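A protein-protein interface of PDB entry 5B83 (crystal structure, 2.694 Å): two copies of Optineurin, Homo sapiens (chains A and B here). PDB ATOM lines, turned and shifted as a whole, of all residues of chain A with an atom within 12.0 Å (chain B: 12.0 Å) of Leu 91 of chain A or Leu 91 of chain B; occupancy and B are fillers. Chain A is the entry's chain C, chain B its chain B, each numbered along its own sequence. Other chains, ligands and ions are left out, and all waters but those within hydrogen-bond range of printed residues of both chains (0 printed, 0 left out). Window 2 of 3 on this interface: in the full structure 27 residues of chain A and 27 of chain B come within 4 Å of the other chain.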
ATOM      1  N   LYS A  81     -14.108  38.090 -22.116  1.00  0.00           N
ATOM      2  CA  LYS A  81     -14.277  36.688 -21.725  1.00  0.00           C
ATOM      3  C   LYS A  81     -15.514  36.500 -20.855  1.00  0.00           C
ATOM      4  O   LYS A  81     -16.267  35.538 -21.054  1.00  0.00           O
ATOM      5  CB  LYS A  81     -13.041  36.155 -20.989  1.00  0.00           C
ATOM      6  CG  LYS A  81     -12.024  35.380 -21.831  1.00  0.00           C
ATOM      7  CD  LYS A  81     -11.388  34.258 -20.992  1.00  0.00           C
ATOM      8  CE  LYS A  81     -10.712  34.838 -19.740  1.00  0.00           C
ATOM      9  NZ  LYS A  81     -10.238  33.854 -18.711  1.00  0.00           N
ATOM     10  N   GLU A  82     -15.759  37.420 -19.898  1.00  0.00           N
ATOM     11  CA  GLU A  82     -16.953  37.306 -19.062  1.00  0.00           C
ATOM     12  C   GLU A  82     -18.245  37.453 -19.854  1.00  0.00           C
ATOM     13  O   GLU A  82     -19.223  36.757 -19.557  1.00  0.00           O
ATOM     14  CB  GLU A  82     -16.925  38.332 -17.941  1.00  0.00           C
ATOM     15  CG  GLU A  82     -15.739  38.151 -17.024  1.00  0.00           C
ATOM     16  CD  GLU A  82     -15.739  39.150 -15.898  1.00  0.00           C
ATOM     17  OE1 GLU A  82     -16.286  40.255 -16.095  1.00  0.00           O
ATOM     18  OE2 GLU A  82     -15.205  38.820 -14.817  1.00  0.00           O
ATOM     19  N   GLN A  83     -18.274  38.320 -20.867  1.00  0.00           N
ATOM     20  CA  GLN A  83     -19.489  38.440 -21.669  1.00  0.00           C
ATOM     21  C   GLN A  83     -19.747  37.148 -22.447  1.00  0.00           C
ATOM     22  O   GLN A  83     -20.872  36.624 -22.456  1.00  0.00           O
ATOM     23  CB  GLN A  83     -19.396  39.660 -22.599  1.00  0.00           C
ATOM     24  CG  GLN A  83     -18.810  40.917 -21.940  1.00  0.00           C
ATOM     25  CD  GLN A  83     -18.275  41.975 -22.940  1.00  0.00           C
ATOM     26  OE1 GLN A  83     -18.391  41.814 -24.161  1.00  0.00           O
ATOM     27  NE2 GLN A  83     -17.686  43.060 -22.411  1.00  0.00           N
ATOM     28  N   LEU A  84     -18.698  36.598 -23.069  1.00  0.00           N
ATOM     29  CA  LEU A  84     -18.825  35.332 -23.789  1.00  0.00           C
ATOM     30  C   LEU A  84     -19.291  34.221 -22.868  1.00  0.00           C
ATOM     31  O   LEU A  84     -20.117  33.382 -23.250  1.00  0.00           O
ATOM     32  CB  LEU A  84     -17.492  34.952 -24.423  1.00  0.00           C
ATOM     33  CG  LEU A  84     -17.095  35.919 -25.539  1.00  0.00           C
ATOM     34  CD1 LEU A  84     -15.833  35.433 -26.286  1.00  0.00           C
ATOM     35  CD2 LEU A  84     -18.313  36.260 -26.524  1.00  0.00           C
ATOM     36  N   ALA A  85     -18.767  34.190 -21.653  1.00  0.00           N
ATOM     37  CA  ALA A  85     -19.108  33.093 -20.771  1.00  0.00           C
ATOM     38  C   ALA A  85     -20.512  33.254 -20.229  1.00  0.00           C
ATOM     39  O   ALA A  85     -21.198  32.246 -20.011  1.00  0.00           O
ATOM     40  CB  ALA A  85     -18.090  33.001 -19.644  1.00  0.00           C
ATOM     41  N   LEU A  86     -20.946  34.503 -20.000  1.00  0.00           N
ATOM     42  CA  LEU A  86     -22.362  34.767 -19.732  1.00  0.00           C
ATOM     43  C   LEU A  86     -23.244  34.340 -20.908  1.00  0.00           C
ATOM     44  O   LEU A  86     -24.295  33.718 -20.715  1.00  0.00           O
ATOM     45  CB  LEU A  86     -22.580  36.253 -19.424  1.00  0.00           C
ATOM     46  CG  LEU A  86     -24.073  36.648 -19.296  1.00  0.00           C
ATOM     47  CD1 LEU A  86     -24.565  36.389 -17.898  1.00  0.00           C
ATOM     48  CD2 LEU A  86     -24.381  38.079 -19.728  1.00  0.00           C
ATOM     49  N   GLN A  87     -22.847  34.704 -22.131  1.00  0.00           N
ATOM     50  CA  GLN A  87     -23.573  34.248 -23.312  1.00  0.00           C
ATOM     51  C   GLN A  87     -23.773  32.743 -23.308  1.00  0.00           C
ATOM     52  O   GLN A  87     -24.857  32.245 -23.657  1.00  0.00           O
ATOM     53  CB  GLN A  87     -22.824  34.620 -24.587  1.00  0.00           C
ATOM     54  CG  GLN A  87     -23.084  35.967 -25.168  1.00  0.00           C
ATOM     55  CD  GLN A  87     -22.550  36.053 -26.581  1.00  0.00           C
ATOM     56  OE1 GLN A  87     -22.803  35.170 -27.401  1.00  0.00           O
ATOM     57  NE2 GLN A  87     -21.797  37.110 -26.872  1.00  0.00           N
ATOM     58  N   LEU A  88     -22.720  31.998 -22.960  1.00  0.00           N
ATOM     59  CA  LEU A  88     -22.802  30.548 -22.967  1.00  0.00           C
ATOM     60  C   LEU A  88     -23.738  30.048 -21.870  1.00  0.00           C
ATOM     61  O   LEU A  88     -24.611  29.216 -22.131  1.00  0.00           O
ATOM     62  CB  LEU A  88     -21.417  29.958 -22.822  1.00  0.00           C
ATOM     63  CG  LEU A  88     -21.288  28.441 -22.846  1.00  0.00           C
ATOM     64  CD1 LEU A  88     -21.220  27.918 -24.273  1.00  0.00           C
ATOM     65  CD2 LEU A  88     -20.048  28.054 -22.106  1.00  0.00           C
ATOM     66  N   ALA A  89     -23.604  30.577 -20.643  1.00  0.00           N
ATOM     67  CA  ALA A  89     -24.505  30.165 -19.568  1.00  0.00           C
ATOM     68  C   ALA A  89     -25.952  30.444 -19.925  1.00  0.00           C
ATOM     69  O   ALA A  89     -26.841  29.668 -19.573  1.00  0.00           O
ATOM     70  CB  ALA A  89     -24.167  30.858 -18.252  1.00  0.00           C
ATOM     71  N   VAL A  90     -26.222  31.546 -20.602  1.00  0.00           N
ATOM     72  CA  VAL A  90     -27.631  31.813 -20.853  1.00  0.00           C
ATOM     73  C   VAL A  90     -28.154  30.869 -21.933  1.00  0.00           C
ATOM     74  O   VAL A  90     -29.234  30.283 -21.792  1.00  0.00           O
ATOM     75  CB  VAL A  90     -27.882  33.308 -21.178  1.00  0.00           C
ATOM     76  CG1 VAL A  90     -29.301  33.523 -21.680  1.00  0.00           C
ATOM     77  CG2 VAL A  90     -27.653  34.191 -19.939  1.00  0.00           C
ATOM     78  N   LEU A  91     -27.387  30.651 -22.997  1.00  0.00           N
ATOM     79  CA  LEU A  91     -27.870  29.773 -24.053  1.00  0.00           C
ATOM     80  C   LEU A  91     -28.136  28.373 -23.531  1.00  0.00           C
ATOM     81  O   LEU A  91     -29.164  27.766 -23.859  1.00  0.00           O
ATOM     82  CB  LEU A  91     -26.869  29.729 -25.192  1.00  0.00           C
ATOM     83  CG  LEU A  91     -26.860  31.043 -25.927  1.00  0.00           C
ATOM     84  CD1 LEU A  91     -25.711  31.094 -26.879  1.00  0.00           C
ATOM     85  CD2 LEU A  91     -28.195  31.170 -26.655  1.00  0.00           C
ATOM     86  N   LEU A  92     -27.225  27.846 -22.713  1.00  0.00           N
ATOM     87  CA  LEU A  92     -27.397  26.503 -22.176  1.00  0.00           C
ATOM     88  C   LEU A  92     -28.555  26.447 -21.194  1.00  0.00           C
ATOM     89  O   LEU A  92     -29.343  25.497 -21.216  1.00  0.00           O
ATOM     90  CB  LEU A  92     -26.100  26.034 -21.515  1.00  0.00           C
ATOM     91  CG  LEU A  92     -24.954  25.812 -22.510  1.00  0.00           C
ATOM     92  CD1 LEU A  92     -23.596  25.871 -21.838  1.00  0.00           C
ATOM     93  CD2 LEU A  92     -25.134  24.497 -23.207  1.00  0.00           C
ATOM     94  N   LYS A  93     -28.681  27.449 -20.326  1.00  0.00           N
ATOM     95  CA  LYS A  93     -29.716  27.384 -19.309  1.00  0.00           C
ATOM     96  C   LYS A  93     -31.106  27.399 -19.943  1.00  0.00           C
ATOM     97  O   LYS A  93     -31.999  26.643 -19.532  1.00  0.00           O
ATOM     98  CB  LYS A  93     -29.544  28.538 -18.334  1.00  0.00           C
ATOM     99  CG  LYS A  93     -30.414  28.460 -17.099  1.00  0.00           C
ATOM    100  CD  LYS A  93     -30.480  29.822 -16.412  1.00  0.00           C
ATOM    101  CE  LYS A  93     -31.696  30.595 -16.888  1.00  0.00           C
ATOM    102  NZ  LYS A  93     -32.925  29.753 -16.736  1.00  0.00           N
ATOM    103  N   GLU A  94     -31.293  28.236 -20.963  1.00  0.00           N
ATOM    104  CA  GLU A  94     -32.590  28.423 -21.596  1.00  0.00           C
ATOM    105  C   GLU A  94     -32.879  27.374 -22.655  1.00  0.00           C
ATOM    106  O   GLU A  94     -34.027  27.245 -23.082  1.00  0.00           O
ATOM    107  CB  GLU A  94     -32.685  29.832 -22.179  1.00  0.00           C
ATOM    108  CG  GLU A  94     -32.823  30.864 -21.072  1.00  0.00           C
ATOM    109  CD  GLU A  94     -32.741  32.281 -21.562  1.00  0.00           C
ATOM    110  OE1 GLU A  94     -32.695  32.496 -22.789  1.00  0.00           O
ATOM    111  OE2 GLU A  94     -32.721  33.183 -20.710  1.00  0.00           O
ATOM    112  N   ASN A  95     -31.866  26.609 -23.062  1.00  0.00           N
ATOM    113  CA  ASN A  95     -32.092  25.409 -23.837  1.00  0.00           C
ATOM    114  C   ASN A  95     -32.720  24.291 -23.012  1.00  0.00           C
ATOM    115  O   ASN A  95     -33.151  23.287 -23.590  1.00  0.00           O
ATOM    116  CB  ASN A  95     -30.764  24.966 -24.437  1.00  0.00           C
ATOM    117  CG  ASN A  95     -30.930  24.336 -25.799  1.00  0.00           C
ATOM    118  OD1 ASN A  95     -30.427  23.249 -26.049  1.00  0.00           O
ATOM    119  ND2 ASN A  95     -31.651  25.024 -26.693  1.00  0.00           N
ATOM    120  N   ASP A  96     -32.817  24.460 -21.683  1.00  0.00           N
ATOM    121  CA  ASP A  96     -33.238  23.409 -20.750  1.00  0.00           C
ATOM    122  C   ASP A  96     -34.281  23.981 -19.789  1.00  0.00           C
ATOM    123  O   ASP A  96     -34.033  24.097 -18.584  1.00  0.00           O
ATOM    124  CB  ASP A  96     -32.035  22.854 -19.982  1.00  0.00           C
ATOM    125  CG  ASP A  96     -31.957  21.346 -20.027  1.00  0.00           C
ATOM    126  OD1 ASP A  96     -31.752  20.808 -21.135  1.00  0.00           O
ATOM    127  OD2 ASP A  96     -32.070  20.702 -18.958  1.00  0.00           O
ATOM    128  N   ALA A  97     -35.445  24.344 -20.325  1.00  0.00           N
ATOM    129  CA  ALA A  97     -36.547  24.797 -19.483  1.00  0.00           C
ATOM    130  C   ALA A  97     -37.899  24.357 -20.053  1.00  0.00           C
ATOM    131  O   ALA A  97     -38.058  23.224 -20.521  1.00  0.00           O
ATOM    132  CB  ALA A  97     -36.490  26.308 -19.310  1.00  0.00           C
ATOM    133  N   GLU B  82     -10.519  33.246 -27.269  1.00  0.00           N
ATOM    134  CA  GLU B  82     -10.820  32.595 -28.536  1.00  0.00           C
ATOM    135  C   GLU B  82     -11.390  31.197 -28.346  1.00  0.00           C
ATOM    136  O   GLU B  82     -12.082  30.696 -29.233  1.00  0.00           O
ATOM    137  CB  GLU B  82      -9.570  32.552 -29.408  1.00  0.00           C
ATOM    138  CG  GLU B  82      -9.298  33.862 -30.107  1.00  0.00           C
ATOM    139  CD  GLU B  82     -10.387  34.228 -31.123  1.00  0.00           C
ATOM    140  OE1 GLU B  82     -11.239  35.109 -30.828  1.00  0.00           O
ATOM    141  OE2 GLU B  82     -10.381  33.618 -32.219  1.00  0.00           O
ATOM    142  N   GLN B  83     -11.104  30.546 -27.215  1.00  0.00           N
ATOM    143  CA  GLN B  83     -11.628  29.201 -26.994  1.00  0.00           C
ATOM    144  C   GLN B  83     -13.104  29.239 -26.580  1.00  0.00           C
ATOM    145  O   GLN B  83     -13.889  28.379 -26.990  1.00  0.00           O
ATOM    146  CB  GLN B  83     -10.757  28.481 -25.957  1.00  0.00           C
ATOM    147  CG  GLN B  83     -10.332  27.033 -26.286  1.00  0.00           C
ATOM    148  CD  GLN B  83      -9.340  26.922 -27.452  1.00  0.00           C
ATOM    149  OE1 GLN B  83      -8.516  27.811 -27.657  1.00  0.00           O
ATOM    150  NE2 GLN B  83      -9.424  25.833 -28.223  1.00  0.00           N
ATOM    151  N   LEU B  84     -13.516  30.236 -25.793  1.00  0.00           N
ATOM    152  CA  LEU B  84     -14.946  30.427 -25.544  1.00  0.00           C
ATOM    153  C   LEU B  84     -15.681  30.772 -26.831  1.00  0.00           C
ATOM    154  O   LEU B  84     -16.772  30.261 -27.089  1.00  0.00           O
ATOM    155  CB  LEU B  84     -15.169  31.537 -24.515  1.00  0.00           C
ATOM    156  CG  LEU B  84     -15.015  31.153 -23.050  1.00  0.00           C
ATOM    157  CD1 LEU B  84     -14.980  32.387 -22.233  1.00  0.00           C
ATOM    158  CD2 LEU B  84     -16.181  30.311 -22.602  1.00  0.00           C
ATOM    159  N   ALA B  85     -15.098  31.648 -27.640  1.00  0.00           N
ATOM    160  CA  ALA B  85     -15.757  32.094 -28.846  1.00  0.00           C
ATOM    161  C   ALA B  85     -16.028  30.913 -29.763  1.00  0.00           C
ATOM    162  O   ALA B  85     -17.120  30.786 -30.333  1.00  0.00           O
ATOM    163  CB  ALA B  85     -14.884  33.140 -29.529  1.00  0.00           C
ATOM    164  N   LEU B  86     -15.042  30.023 -29.870  1.00  0.00           N
ATOM    165  CA  LEU B  86     -15.184  28.778 -30.597  1.00  0.00           C
ATOM    166  C   LEU B  86     -16.376  28.007 -30.074  1.00  0.00           C
ATOM    167  O   LEU B  86     -17.326  27.720 -30.817  1.00  0.00           O
ATOM    168  CB  LEU B  86     -13.898  27.952 -30.448  1.00  0.00           C
ATOM    169  CG  LEU B  86     -13.877  26.647 -31.240  1.00  0.00           C
ATOM    170  CD1 LEU B  86     -13.729  26.892 -32.740  1.00  0.00           C
ATOM    171  CD2 LEU B  86     -12.801  25.684 -30.717  1.00  0.00           C
ATOM    172  N   GLN B  87     -16.355  27.695 -28.773  1.00  0.00           N
ATOM    173  CA  GLN B  87     -17.443  26.925 -28.186  1.00  0.00           C
ATOM    174  C   GLN B  87     -18.800  27.571 -28.451  1.00  0.00           C
ATOM    175  O   GLN B  87     -19.811  26.864 -28.587  1.00  0.00           O
ATOM    176  CB  GLN B  87     -17.219  26.736 -26.689  1.00  0.00           C
ATOM    177  CG  GLN B  87     -18.377  26.083 -25.982  1.00  0.00           C
ATOM    178  CD  GLN B  87     -18.633  24.648 -26.427  1.00  0.00           C
ATOM    179  OE1 GLN B  87     -18.193  23.707 -25.777  1.00  0.00           O
ATOM    180  NE2 GLN B  87     -19.387  24.475 -27.510  1.00  0.00           N
ATOM    181  N   LEU B  88     -18.840  28.901 -28.577  1.00  0.00           N
ATOM    182  CA  LEU B  88     -20.094  29.559 -28.944  1.00  0.00           C
ATOM    183  C   LEU B  88     -20.455  29.283 -30.395  1.00  0.00           C
ATOM    184  O   LEU B  88     -21.566  28.825 -30.695  1.00  0.00           O
ATOM    185  CB  LEU B  88     -19.993  31.051 -28.725  1.00  0.00           C
ATOM    186  CG  LEU B  88     -20.236  31.531 -27.325  1.00  0.00           C
ATOM    187  CD1 LEU B  88     -20.189  33.033 -27.462  1.00  0.00           C
ATOM    188  CD2 LEU B  88     -21.573  31.014 -26.834  1.00  0.00           C
ATOM    189  N   ALA B  89     -19.523  29.579 -31.303  1.00  0.00           N
ATOM    190  CA  ALA B  89     -19.695  29.322 -32.729  1.00  0.00           C
ATOM    191  C   ALA B  89     -20.192  27.904 -33.021  1.00  0.00           C
ATOM    192  O   ALA B  89     -21.065  27.707 -33.884  1.00  0.00           O
ATOM    193  CB  ALA B  89     -18.363  29.588 -33.429  1.00  0.00           C
ATOM    194  N   VAL B  90     -19.669  26.914 -32.288  1.00  0.00           N
ATOM    195  CA  VAL B  90     -19.925  25.488 -32.510  1.00  0.00           C
ATOM    196  C   VAL B  90     -21.201  24.997 -31.839  1.00  0.00           C
ATOM    197  O   VAL B  90     -21.523  23.808 -31.904  1.00  0.00           O
ATOM    198  CB  VAL B  90     -18.616  24.796 -32.039  1.00  0.00           C
ATOM    199  CG1 VAL B  90     -18.804  23.466 -31.362  1.00  0.00           C
ATOM    200  CG2 VAL B  90     -17.656  24.645 -33.150  1.00  0.00           C
ATOM    201  N   LEU B  91     -21.979  25.872 -31.224  1.00  0.00           N
ATOM    202  CA  LEU B  91     -23.084  25.404 -30.384  1.00  0.00           C
ATOM    203  C   LEU B  91     -24.190  24.670 -31.135  1.00  0.00           C
ATOM    204  O   LEU B  91     -25.154  24.225 -30.508  1.00  0.00           O
ATOM    205  CB  LEU B  91     -23.713  26.578 -29.643  1.00  0.00           C
ATOM    206  CG  LEU B  91     -23.166  26.963 -28.286  1.00  0.00           C
ATOM    207  CD1 LEU B  91     -23.837  28.228 -27.870  1.00  0.00           C
ATOM    208  CD2 LEU B  91     -23.465  25.887 -27.277  1.00  0.00           C
ATOM    209  N   LEU B  92     -24.068  24.562 -32.461  1.00  0.00           N
ATOM    210  CA  LEU B  92     -25.024  23.886 -33.323  1.00  0.00           C
ATOM    211  C   LEU B  92     -24.285  23.073 -34.387  1.00  0.00           C
ATOM    212  O   LEU B  92     -23.208  23.463 -34.853  1.00  0.00           O
ATOM    213  CB  LEU B  92     -25.941  24.911 -33.970  1.00  0.00           C
ATOM    214  CG  LEU B  92     -26.692  25.851 -33.015  1.00  0.00           C
ATOM    215  CD1 LEU B  92     -27.567  26.753 -33.826  1.00  0.00           C
ATOM    216  CD2 LEU B  92     -27.575  25.078 -32.092  1.00  0.00           C
ATOM    217  N   LYS B  93     -24.874  21.939 -34.777  1.00  0.00           N
ATOM    218  CA  LYS B  93     -24.180  20.999 -35.668  1.00  0.00           C
ATOM    219  C   LYS B  93     -24.945  19.734 -36.031  1.00  0.00           C
ATOM    220  O   LYS B  93     -24.325  18.739 -36.436  1.00  0.00           O
ATOM    221  CB  LYS B  93     -22.858  20.572 -35.051  1.00  0.00           C
ATOM    222  CG  LYS B  93     -21.680  21.114 -35.800  1.00  0.00           C
ATOM    223  CD  LYS B  93     -20.384  20.523 -35.310  1.00  0.00           C
ATOM    224  CE  LYS B  93     -19.235  21.403 -35.741  1.00  0.00           C
ATOM    225  NZ  LYS B  93     -17.957  21.005 -35.098  1.00  0.00           N
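Leu 84 of chain B touches Lys 81 of chain A. Leu 88 of chain B touches Leu 84 of chain A (CD1 to CD2, 3.8 Å). Leu 88 of chain B touches Gln 87 of chain A. Leu 88 of chain A touches Gln 87 of chain B (CD1 to CG, 3.8 Å). CD1 of Leu 91 of chain B touches CD1 of Leu 91 of chain A, 3.6 Å away.
Printed residues of chain B within 4 Å of Lys 81 of chain A: Leu 84 (3.6 Å). Of the printed residues of chain B, Leu 84 of chain A touches Leu 88. Of chain B, only Gln 87 comes within 4 Å of Leu 88 of chain A. No residue of chain B comes within 4 Å of Val 90 of chain A. Leu 91 of chain A touches one residue of chain B. No residue of chain B comes within 4 Å of Glu 94 of chain A. No residue of chain B comes within 4 Å of Asn 95 of chain A. Ala 97 of chain A touches none of the printed residues of chain B. Of the printed residues of chain A, Leu 84 of chain B touches Lys 81 (3.6 Å). Gln 87 of chain B touches one residue of chain A. Leu 88 of chain B touches two residues of chain A. No residue of chain A comes within 4 Å of Ala 89 of chain B. No residue of chain A comes within 4 Å of Val 90 of chain B. Leu 91 of chain B touches one residue of chain A. No residue of chain A comes within 4 Å of Leu 92 of chain B. The nearest residue of chain A that does not touch Leu 91 of chain B is Leu 88 of chain A (4.3 Å). The nearest printed residue of chain B that does not touch Leu 84 of chain A is Ala 85 of chain B (4.1 Å).
Of the 12 printed residues of chain B, 4 touch a printed residue of chain A. Of the 17 printed residues of chain A, 5 touch a printed residue of chain B. Hydrophobic or aromatic side chains of chain A that line the printed part of chain B: Leu 84, Leu 88 and Leu 91. Among the printed residues, no Asp or Glu carboxylate lies within 4 Å of a Lys or Arg side-chain nitrogen of the other chain.
Leu 84 of chain A touches Leu 88 of chain B, but with the chains exchanged Leu 88 of chain A does not touch Leu 84 of chain B (4.5 Å). Gln 87 of chain A touches Leu 88 of chain B, and with the chains exchanged Leu 88 of chain A touches Gln 87 of chain B. Leu 91 of chain A touches its own counterpart, Leu 91 of chain B. Positions printed for both chains: 82, 83, 84, 85, 86, 87, 88, 89, 90, 91, 92 and 93.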
